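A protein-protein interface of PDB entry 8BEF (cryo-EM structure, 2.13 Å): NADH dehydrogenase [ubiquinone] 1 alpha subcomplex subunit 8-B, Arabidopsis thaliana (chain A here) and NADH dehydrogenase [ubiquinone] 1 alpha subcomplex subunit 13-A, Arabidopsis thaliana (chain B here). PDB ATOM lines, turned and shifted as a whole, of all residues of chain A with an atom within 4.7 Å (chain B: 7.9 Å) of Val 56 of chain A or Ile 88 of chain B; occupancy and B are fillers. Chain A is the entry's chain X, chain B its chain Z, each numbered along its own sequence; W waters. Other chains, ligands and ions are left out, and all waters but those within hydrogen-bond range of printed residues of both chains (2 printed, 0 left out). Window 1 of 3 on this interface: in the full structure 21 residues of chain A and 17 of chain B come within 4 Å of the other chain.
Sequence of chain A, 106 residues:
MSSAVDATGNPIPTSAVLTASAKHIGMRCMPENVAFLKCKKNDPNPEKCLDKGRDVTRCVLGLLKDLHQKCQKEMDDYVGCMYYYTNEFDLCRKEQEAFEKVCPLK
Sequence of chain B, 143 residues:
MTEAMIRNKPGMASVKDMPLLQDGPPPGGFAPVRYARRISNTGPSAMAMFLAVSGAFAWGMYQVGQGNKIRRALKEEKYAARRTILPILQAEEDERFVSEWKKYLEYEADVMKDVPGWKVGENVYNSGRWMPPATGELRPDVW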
ATOM      1  N   LEU A  18      16.101  15.347   9.214  1.00  0.00           N
ATOM      2  CA  LEU A  18      15.387  16.249   8.317  1.00  0.00           C
ATOM      3  C   LEU A  18      15.623  17.707   8.693  1.00  0.00           C
ATOM      4  O   LEU A  18      15.868  18.546   7.824  1.00  0.00           O
ATOM      5  CB  LEU A  18      13.895  15.920   8.325  1.00  0.00           C
ATOM      6  CG  LEU A  18      13.548  14.530   7.785  1.00  0.00           C
ATOM      7  CD1 LEU A  18      12.091  14.188   8.047  1.00  0.00           C
ATOM      8  CD2 LEU A  18      13.869  14.448   6.302  1.00  0.00           C
ATOM      9  N   GLU A  32       9.371  20.020  -6.360  1.00  0.00           N
ATOM     10  CA  GLU A  32       8.483  18.994  -5.823  1.00  0.00           C
ATOM     11  C   GLU A  32       7.701  19.516  -4.625  1.00  0.00           C
ATOM     12  O   GLU A  32       6.496  19.257  -4.499  1.00  0.00           O
ATOM     13  CB  GLU A  32       9.286  17.754  -5.432  1.00  0.00           C
ATOM     14  CG  GLU A  32       9.785  16.928  -6.600  1.00  0.00           C
ATOM     15  CD  GLU A  32      11.056  17.485  -7.209  1.00  0.00           C
ATOM     16  OE1 GLU A  32      11.596  18.472  -6.669  1.00  0.00           O
ATOM     17  OE2 GLU A  32      11.515  16.935  -8.233  1.00  0.00           O
ATOM     18  N   ASN A  33       8.371  20.254  -3.737  1.00  0.00           N
ATOM     19  CA  ASN A  33       7.702  20.827  -2.573  1.00  0.00           C
ATOM     20  C   ASN A  33       6.573  21.758  -2.998  1.00  0.00           C
ATOM     21  O   ASN A  33       5.446  21.657  -2.499  1.00  0.00           O
ATOM     22  CB  ASN A  33       8.718  21.583  -1.710  1.00  0.00           C
ATOM     23  CG  ASN A  33       9.503  20.670  -0.782  1.00  0.00           C
ATOM     24  OD1 ASN A  33       9.228  19.476  -0.680  1.00  0.00           O
ATOM     25  ND2 ASN A  33      10.491  21.235  -0.102  1.00  0.00           N
ATOM     26  N   PHE A  36       3.624  19.804  -4.541  1.00  0.00           N
ATOM     27  CA  PHE A  36       2.859  19.143  -3.491  1.00  0.00           C
ATOM     28  C   PHE A  36       1.977  20.139  -2.751  1.00  0.00           C
ATOM     29  O   PHE A  36       0.806  19.861  -2.470  1.00  0.00           O
ATOM     30  CB  PHE A  36       3.812  18.445  -2.520  1.00  0.00           C
ATOM     31  CG  PHE A  36       3.124  17.741  -1.389  1.00  0.00           C
ATOM     32  CD1 PHE A  36       2.575  16.483  -1.565  1.00  0.00           C
ATOM     33  CD2 PHE A  36       3.021  18.343  -0.142  1.00  0.00           C
ATOM     34  CE1 PHE A  36       1.946  15.835  -0.520  1.00  0.00           C
ATOM     35  CE2 PHE A  36       2.387  17.700   0.902  1.00  0.00           C
ATOM     36  CZ  PHE A  36       1.849  16.444   0.712  1.00  0.00           C
ATOM     37  N   LYS A  52       2.274  13.302  -6.034  1.00  0.00           N
ATOM     38  CA  LYS A  52       3.167  14.399  -5.678  1.00  0.00           C
ATOM     39  C   LYS A  52       3.923  14.093  -4.395  1.00  0.00           C
ATOM     40  O   LYS A  52       5.097  14.463  -4.258  1.00  0.00           O
ATOM     41  CB  LYS A  52       2.373  15.699  -5.539  1.00  0.00           C
ATOM     42  CG  LYS A  52       2.381  16.561  -6.785  1.00  0.00           C
ATOM     43  CD  LYS A  52       1.246  16.184  -7.716  1.00  0.00           C
ATOM     44  CE  LYS A  52       1.310  16.969  -9.015  1.00  0.00           C
ATOM     45  NZ  LYS A  52       1.096  18.424  -8.796  1.00  0.00           N
ATOM     46  N   GLY A  53       3.275  13.402  -3.456  1.00  0.00           N
ATOM     47  CA  GLY A  53       3.965  12.981  -2.251  1.00  0.00           C
ATOM     48  C   GLY A  53       5.109  12.027  -2.535  1.00  0.00           C
ATOM     49  O   GLY A  53       6.178  12.129  -1.930  1.00  0.00           O
ATOM     50  N   ARG A  54       4.899  11.084  -3.457  1.00  0.00           N
ATOM     51  CA  ARG A  54       5.975  10.171  -3.832  1.00  0.00           C
ATOM     52  C   ARG A  54       7.127  10.919  -4.491  1.00  0.00           C
ATOM     53  O   ARG A  54       8.298  10.621  -4.231  1.00  0.00           O
ATOM     54  CB  ARG A  54       5.441   9.072  -4.752  1.00  0.00           C
ATOM     55  CG  ARG A  54       4.508   8.091  -4.060  1.00  0.00           C
ATOM     56  CD  ARG A  54       4.100   6.949  -4.978  1.00  0.00           C
ATOM     57  NE  ARG A  54       2.891   7.256  -5.735  1.00  0.00           N
ATOM     58  CZ  ARG A  54       1.659   6.982  -5.326  1.00  0.00           C
ATOM     59  NH1 ARG A  54       1.432   6.394  -4.163  1.00  0.00           N
ATOM     60  NH2 ARG A  54       0.630   7.308  -6.103  1.00  0.00           N
ATOM     61  N   ASP A  55       6.813  11.895  -5.347  1.00  0.00           N
ATOM     62  CA  ASP A  55       7.867  12.720  -5.942  1.00  0.00           C
ATOM     63  C   ASP A  55       8.679  13.437  -4.866  1.00  0.00           C
ATOM     64  O   ASP A  55       9.921  13.421  -4.885  1.00  0.00           O
ATOM     65  CB  ASP A  55       7.261  13.728  -6.921  1.00  0.00           C
ATOM     66  CG  ASP A  55       6.417  13.068  -7.994  1.00  0.00           C
ATOM     67  OD1 ASP A  55       6.025  13.764  -8.954  1.00  0.00           O
ATOM     68  OD2 ASP A  55       6.163  11.850  -7.891  1.00  0.00           O
ATOM     69  N   VAL A  56       7.988  14.054  -3.903  1.00  0.00           N
ATOM     70  CA  VAL A  56       8.673  14.741  -2.811  1.00  0.00           C
ATOM     71  C   VAL A  56       9.562  13.766  -2.047  1.00  0.00           C
ATOM     72  O   VAL A  56      10.738  14.044  -1.778  1.00  0.00           O
ATOM     73  CB  VAL A  56       7.651  15.417  -1.877  1.00  0.00           C
ATOM     74  CG1 VAL A  56       8.231  15.587  -0.478  1.00  0.00           C
ATOM     75  CG2 VAL A  56       7.205  16.755  -2.435  1.00  0.00           C
ATOM     76  N   THR A  57       9.005  12.604  -1.688  1.00  0.00           N
ATOM     77  CA  THR A  57       9.732  11.644  -0.866  1.00  0.00           C
ATOM     78  C   THR A  57      10.973  11.131  -1.580  1.00  0.00           C
ATOM     79  O   THR A  57      12.039  10.993  -0.969  1.00  0.00           O
ATOM     80  CB  THR A  57       8.816  10.478  -0.491  1.00  0.00           C
ATOM     81  OG1 THR A  57       7.615  10.979   0.108  1.00  0.00           O
ATOM     82  CG2 THR A  57       9.513   9.543   0.485  1.00  0.00           C
ATOM     83  N   ARG A  58      10.853  10.839  -2.876  1.00  0.00           N
ATOM     84  CA  ARG A  58      12.003  10.365  -3.636  1.00  0.00           C
ATOM     85  C   ARG A  58      13.088  11.430  -3.713  1.00  0.00           C
ATOM     86  O   ARG A  58      14.271  11.132  -3.501  1.00  0.00           O
ATOM     87  CB  ARG A  58      11.553   9.937  -5.030  1.00  0.00           C
ATOM     88  CG  ARG A  58      12.623   9.970  -6.092  1.00  0.00           C
ATOM     89  CD  ARG A  58      12.092   9.455  -7.425  1.00  0.00           C
ATOM     90  NE  ARG A  58      10.966   8.541  -7.269  1.00  0.00           N
ATOM     91  CZ  ARG A  58       9.693   8.869  -7.462  1.00  0.00           C
ATOM     92  NH1 ARG A  58       9.341  10.091  -7.822  1.00  0.00           N
ATOM     93  NH2 ARG A  58       8.753   7.945  -7.288  1.00  0.00           N
ATOM     94  N   CYS A  59      12.706  12.682  -3.996  1.00  0.00           N
ATOM     95  CA  CYS A  59      13.696  13.758  -4.012  1.00  0.00           C
ATOM     96  C   CYS A  59      14.427  13.851  -2.676  1.00  0.00           C
ATOM     97  O   CYS A  59      15.663  13.913  -2.630  1.00  0.00           O
ATOM     98  CB  CYS A  59      13.024  15.091  -4.345  1.00  0.00           C
ATOM     99  SG  CYS A  59      14.154  16.506  -4.403  1.00  0.00           S
ATOM    100  N   VAL A  60      13.672  13.844  -1.574  1.00  0.00           N
ATOM    101  CA  VAL A  60      14.273  14.056  -0.260  1.00  0.00           C
ATOM    102  C   VAL A  60      15.188  12.895   0.111  1.00  0.00           C
ATOM    103  O   VAL A  60      16.295  13.102   0.619  1.00  0.00           O
ATOM    104  CB  VAL A  60      13.186  14.280   0.806  1.00  0.00           C
ATOM    105  CG1 VAL A  60      13.825  14.419   2.184  1.00  0.00           C
ATOM    106  CG2 VAL A  60      12.362  15.509   0.475  1.00  0.00           C
ATOM    107  N   ARG B  83       9.383  24.727   7.210  1.00  0.00           N
ATOM    108  CA  ARG B  83       8.632  24.839   5.966  1.00  0.00           C
ATOM    109  C   ARG B  83       9.192  23.934   4.871  1.00  0.00           C
ATOM    110  O   ARG B  83       8.424  23.400   4.066  1.00  0.00           O
ATOM    111  CB  ARG B  83       8.607  26.299   5.511  1.00  0.00           C
ATOM    112  CG  ARG B  83       7.409  27.072   6.043  1.00  0.00           C
ATOM    113  CD  ARG B  83       7.246  28.422   5.364  1.00  0.00           C
ATOM    114  NE  ARG B  83       8.374  29.299   5.648  1.00  0.00           N
ATOM    115  CZ  ARG B  83       8.396  30.205   6.616  1.00  0.00           C
ATOM    116  NH1 ARG B  83       7.345  30.418   7.387  1.00  0.00           N
ATOM    117  NH2 ARG B  83       9.504  30.913   6.815  1.00  0.00           N
ATOM    118  N   THR B  84      10.514  23.739   4.828  1.00  0.00           N
ATOM    119  CA  THR B  84      11.100  22.942   3.752  1.00  0.00           C
ATOM    120  C   THR B  84      10.866  21.446   3.936  1.00  0.00           C
ATOM    121  O   THR B  84      10.792  20.713   2.945  1.00  0.00           O
ATOM    122  CB  THR B  84      12.599  23.219   3.616  1.00  0.00           C
ATOM    123  OG1 THR B  84      13.329  22.430   4.562  1.00  0.00           O
ATOM    124  CG2 THR B  84      12.904  24.684   3.818  1.00  0.00           C
ATOM    125  N   ILE B  85      10.755  20.968   5.178  1.00  0.00           N
ATOM    126  CA  ILE B  85      10.502  19.551   5.423  1.00  0.00           C
ATOM    127  C   ILE B  85       9.028  19.249   5.628  1.00  0.00           C
ATOM    128  O   ILE B  85       8.667  18.088   5.861  1.00  0.00           O
ATOM    129  CB  ILE B  85      11.323  19.031   6.620  1.00  0.00           C
ATOM    130  CG1 ILE B  85      10.847  19.670   7.929  1.00  0.00           C
ATOM    131  CG2 ILE B  85      12.803  19.271   6.395  1.00  0.00           C
ATOM    132  CD1 ILE B  85      11.262  18.909   9.160  1.00  0.00           C
ATOM    133  N   LEU B  86       8.165  20.261   5.548  1.00  0.00           N
ATOM    134  CA  LEU B  86       6.725  20.032   5.655  1.00  0.00           C
ATOM    135  C   LEU B  86       6.200  19.043   4.617  1.00  0.00           C
ATOM    136  O   LEU B  86       5.454  18.123   5.001  1.00  0.00           O
ATOM    137  CB  LEU B  86       6.003  21.383   5.566  1.00  0.00           C
ATOM    138  CG  LEU B  86       4.482  21.492   5.691  1.00  0.00           C
ATOM    139  CD1 LEU B  86       3.775  21.275   4.368  1.00  0.00           C
ATOM    140  CD2 LEU B  86       3.982  20.521   6.700  1.00  0.00           C
ATOM    141  N   PRO B  87       6.511  19.169   3.319  1.00  0.00           N
ATOM    142  CA  PRO B  87       5.883  18.265   2.337  1.00  0.00           C
ATOM    143  C   PRO B  87       6.151  16.787   2.570  1.00  0.00           C
ATOM    144  O   PRO B  87       5.228  15.983   2.411  1.00  0.00           O
ATOM    145  CB  PRO B  87       6.467  18.749   1.003  1.00  0.00           C
ATOM    146  CG  PRO B  87       6.796  20.167   1.244  1.00  0.00           C
ATOM    147  CD  PRO B  87       7.297  20.220   2.645  1.00  0.00           C
ATOM    148  N   ILE B  88       7.368  16.397   2.952  1.00  0.00           N
ATOM    149  CA  ILE B  88       7.647  14.972   3.123  1.00  0.00           C
ATOM    150  C   ILE B  88       6.920  14.419   4.345  1.00  0.00           C
ATOM    151  O   ILE B  88       6.387  13.301   4.315  1.00  0.00           O
ATOM    152  CB  ILE B  88       9.166  14.710   3.182  1.00  0.00           C
ATOM    153  CG1 ILE B  88       9.427  13.201   3.170  1.00  0.00           C
ATOM    154  CG2 ILE B  88       9.814  15.382   4.389  1.00  0.00           C
ATOM    155  CD1 ILE B  88      10.866  12.822   3.342  1.00  0.00           C
ATOM    156  N   LEU B  89       6.864  15.195   5.431  1.00  0.00           N
ATOM    157  CA  LEU B  89       6.102  14.768   6.599  1.00  0.00           C
ATOM    158  C   LEU B  89       4.624  14.618   6.261  1.00  0.00           C
ATOM    159  O   LEU B  89       3.981  13.636   6.657  1.00  0.00           O
ATOM    160  CB  LEU B  89       6.301  15.763   7.742  1.00  0.00           C
ATOM    161  CG  LEU B  89       7.751  15.954   8.198  1.00  0.00           C
ATOM    162  CD1 LEU B  89       7.902  17.199   9.063  1.00  0.00           C
ATOM    163  CD2 LEU B  89       8.252  14.718   8.936  1.00  0.00           C
ATOM    164  N   GLN B  90       4.074  15.575   5.507  1.00  0.00           N
ATOM    165  CA  GLN B  90       2.671  15.489   5.120  1.00  0.00           C
ATOM    166  C   GLN B  90       2.417  14.291   4.212  1.00  0.00           C
ATOM    167  O   GLN B  90       1.386  13.630   4.335  1.00  0.00           O
ATOM    168  CB  GLN B  90       2.228  16.780   4.434  1.00  0.00           C
ATOM    169  CG  GLN B  90       0.736  17.052   4.527  1.00  0.00           C
ATOM    170  CD  GLN B  90       0.152  16.694   5.880  1.00  0.00           C
ATOM    171  OE1 GLN B  90       0.426  17.354   6.879  1.00  0.00           O
ATOM    172  NE2 GLN B  90      -0.665  15.650   5.918  1.00  0.00           N
ATOM    173  N   ALA B  91       3.337  14.007   3.287  1.00  0.00           N
ATOM    174  CA  ALA B  91       3.166  12.866   2.390  1.00  0.00           C
ATOM    175  C   ALA B  91       3.187  11.551   3.160  1.00  0.00           C
ATOM    176  O   ALA B  91       2.375  10.652   2.900  1.00  0.00           O
ATOM    177  CB  ALA B  91       4.255  12.879   1.320  1.00  0.00           C
ATOM    178  N   GLU B  92       4.114  11.423   4.112  1.00  0.00           N
ATOM    179  CA  GLU B  92       4.135  10.255   4.985  1.00  0.00           C
ATOM    180  C   GLU B  92       2.817  10.111   5.736  1.00  0.00           C
ATOM    181  O   GLU B  92       2.239   9.016   5.802  1.00  0.00           O
ATOM    182  CB  GLU B  92       5.298  10.374   5.965  1.00  0.00           C
ATOM    183  CG  GLU B  92       5.465   9.198   6.893  1.00  0.00           C
ATOM    184  CD  GLU B  92       6.608   9.404   7.864  1.00  0.00           C
ATOM    185  OE1 GLU B  92       7.766   9.149   7.481  1.00  0.00           O
ATOM    186  OE2 GLU B  92       6.346   9.819   9.011  1.00  0.00           O
ATOM    187  N   GLU B  93       2.323  11.213   6.307  1.00  0.00           N
ATOM    188  CA  GLU B  93       1.066  11.156   7.044  1.00  0.00           C
ATOM    189  C   GLU B  93      -0.094  10.776   6.130  1.00  0.00           C
ATOM    190  O   GLU B  93      -0.996  10.036   6.535  1.00  0.00           O
ATOM    191  CB  GLU B  93       0.793  12.494   7.735  1.00  0.00           C
ATOM    192  CG  GLU B  93      -0.616  12.629   8.305  1.00  0.00           C
ATOM    193  CD  GLU B  93      -0.888  11.721   9.499  1.00  0.00           C
ATOM    194  OE1 GLU B  93       0.004  10.943   9.899  1.00  0.00           O
ATOM    195  OE2 GLU B  93      -2.014  11.774  10.029  1.00  0.00           O
ATOM    196  N   ASP B  94      -0.086  11.275   4.893  1.00  0.00           N
ATOM    197  CA  ASP B  94      -1.151  10.950   3.951  1.00  0.00           C
ATOM    198  C   ASP B  94      -1.154   9.464   3.621  1.00  0.00           C
ATOM    199  O   ASP B  94      -2.209   8.822   3.609  1.00  0.00           O
ATOM    200  CB  ASP B  94      -0.998  11.783   2.678  1.00  0.00           C
ATOM    201  CG  ASP B  94      -1.489  13.207   2.847  1.00  0.00           C
ATOM    202  OD1 ASP B  94      -2.024  13.530   3.927  1.00  0.00           O
ATOM    203  OD2 ASP B  94      -1.351  13.998   1.892  1.00  0.00           O
ATOM    204  N   GLU B  95       0.025   8.897   3.355  1.00  0.00           N
ATOM    205  CA  GLU B  95       0.100   7.462   3.082  1.00  0.00           C
ATOM    206  C   GLU B  95      -0.378   6.647   4.280  1.00  0.00           C
ATOM    207  O   GLU B  95      -1.159   5.694   4.129  1.00  0.00           O
ATOM    208  CB  GLU B  95       1.530   7.079   2.701  1.00  0.00           C
ATOM    209  CG  GLU B  95       1.902   7.429   1.269  1.00  0.00           C
ATOM    210  CD  GLU B  95       1.447   6.383   0.272  1.00  0.00           C
ATOM    211  OE1 GLU B  95       0.651   5.499   0.650  1.00  0.00           O
ATOM    212  OE2 GLU B  95       1.891   6.439  -0.894  1.00  0.00           O
HETATM  213  O   HOH W   1       9.937  17.989   2.179  1.00  0.00           O
HETATM  214  O   HOH W   2       6.808  10.962   2.706  1.00  0.00           O
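O of Thr 84 of chain B lies within hydrogen-bond range of ND2 of Asn 33 of chain A (3.1 Å). NH1 of Arg 54 of chain A lies within salt-bridge range of OE2 of Glu 95 of chain B (3.3 Å).
Water W2 lies within hydrogen-bond range of OG1 of Thr 57 of chain A, O of Ile 88 of chain B and N of Glu 92 of chain B. Water W1 lies within hydrogen-bond range of O of Thr 84 of chain B, N of Ile 88 of chain B and OD1 of Asn 33 of chain A.
Of the 13 printed residues of chain A, 7 touch a printed residue of chain B. Hydrophobic or aromatic side chains of chain A within 4 Å of the printed part of chain B: Leu 18, Phe 36, Val 56 and Val 60. Of the 13 printed residues of chain B, 8 touch a printed residue of chain A. Hydrophobic or aromatic side chains of chain B within 4 Å of the printed part of chain A: Ile 85, Pro 87, Ile 88, Leu 89 and Ala 91.
Of the printed residues of chain B, Gly 53 of chain A touches Ala 91. Asp 55 of chain A touches none of the printed residues of chain B. Val 56 of chain A touches just these residues of chain B: Pro 87 (3.9 Å) and Ile 88 (3.6 Å). Printed residues of chain A within 4 Å of Thr 84 of chain B: Asn 33. Of chain A, only Val 56 and Val 60 come within 4 Å of Ile 88 of chain B. Glu 93 of chain B touches none of the printed residues of chain A. Of the printed residues of chain A, Glu 95 of chain B touches Arg 54 (3.3 Å). The nearest residue of chain B that does not touch Val 56 of chain A is Ala 91 of chain B (5.1 Å). The nearest printed residue of chain B that does not touch Phe 36 of chain A is Asp 94 of chain B (4.2 Å).
NE2 of Gln 90 of chain B lies within hydrogen-bond range of OD1 of Asp 94 of chain B (3.2 Å). The side-chain hydroxyl of Thr 57 of chain A is in hydrogen-bond range of the backbone carbonyl oxygen of Gly 53 of chain A.
Among the printed residues, pairs that only touch across the chains: Leu 18 of chain A with Ile 85 of chain B (3.5 Å), Leu 18 of chain A with Leu 89 of chain B (3.98 Å), Asn 33 of chain A with Pro 87 of chain B (3.2 Å), Phe 36 of chain A with Pro 87 of chain B (3.6 Å), Phe 36 of chain A with Gln 90 of chain B (3.7 Å), Phe 36 of chain A with Ala 91 of chain B (3.8 Å), Gly 53 of chain A with Ala 91 of chain B (3.6 Å), Val 56 of chain A with Pro 87 of chain B (3.9 Å), Val 56 of chain A with Ile 88 of chain B (3.6 Å) and Val 60 of chain A with Ile 88 of chain B (3.6 Å).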
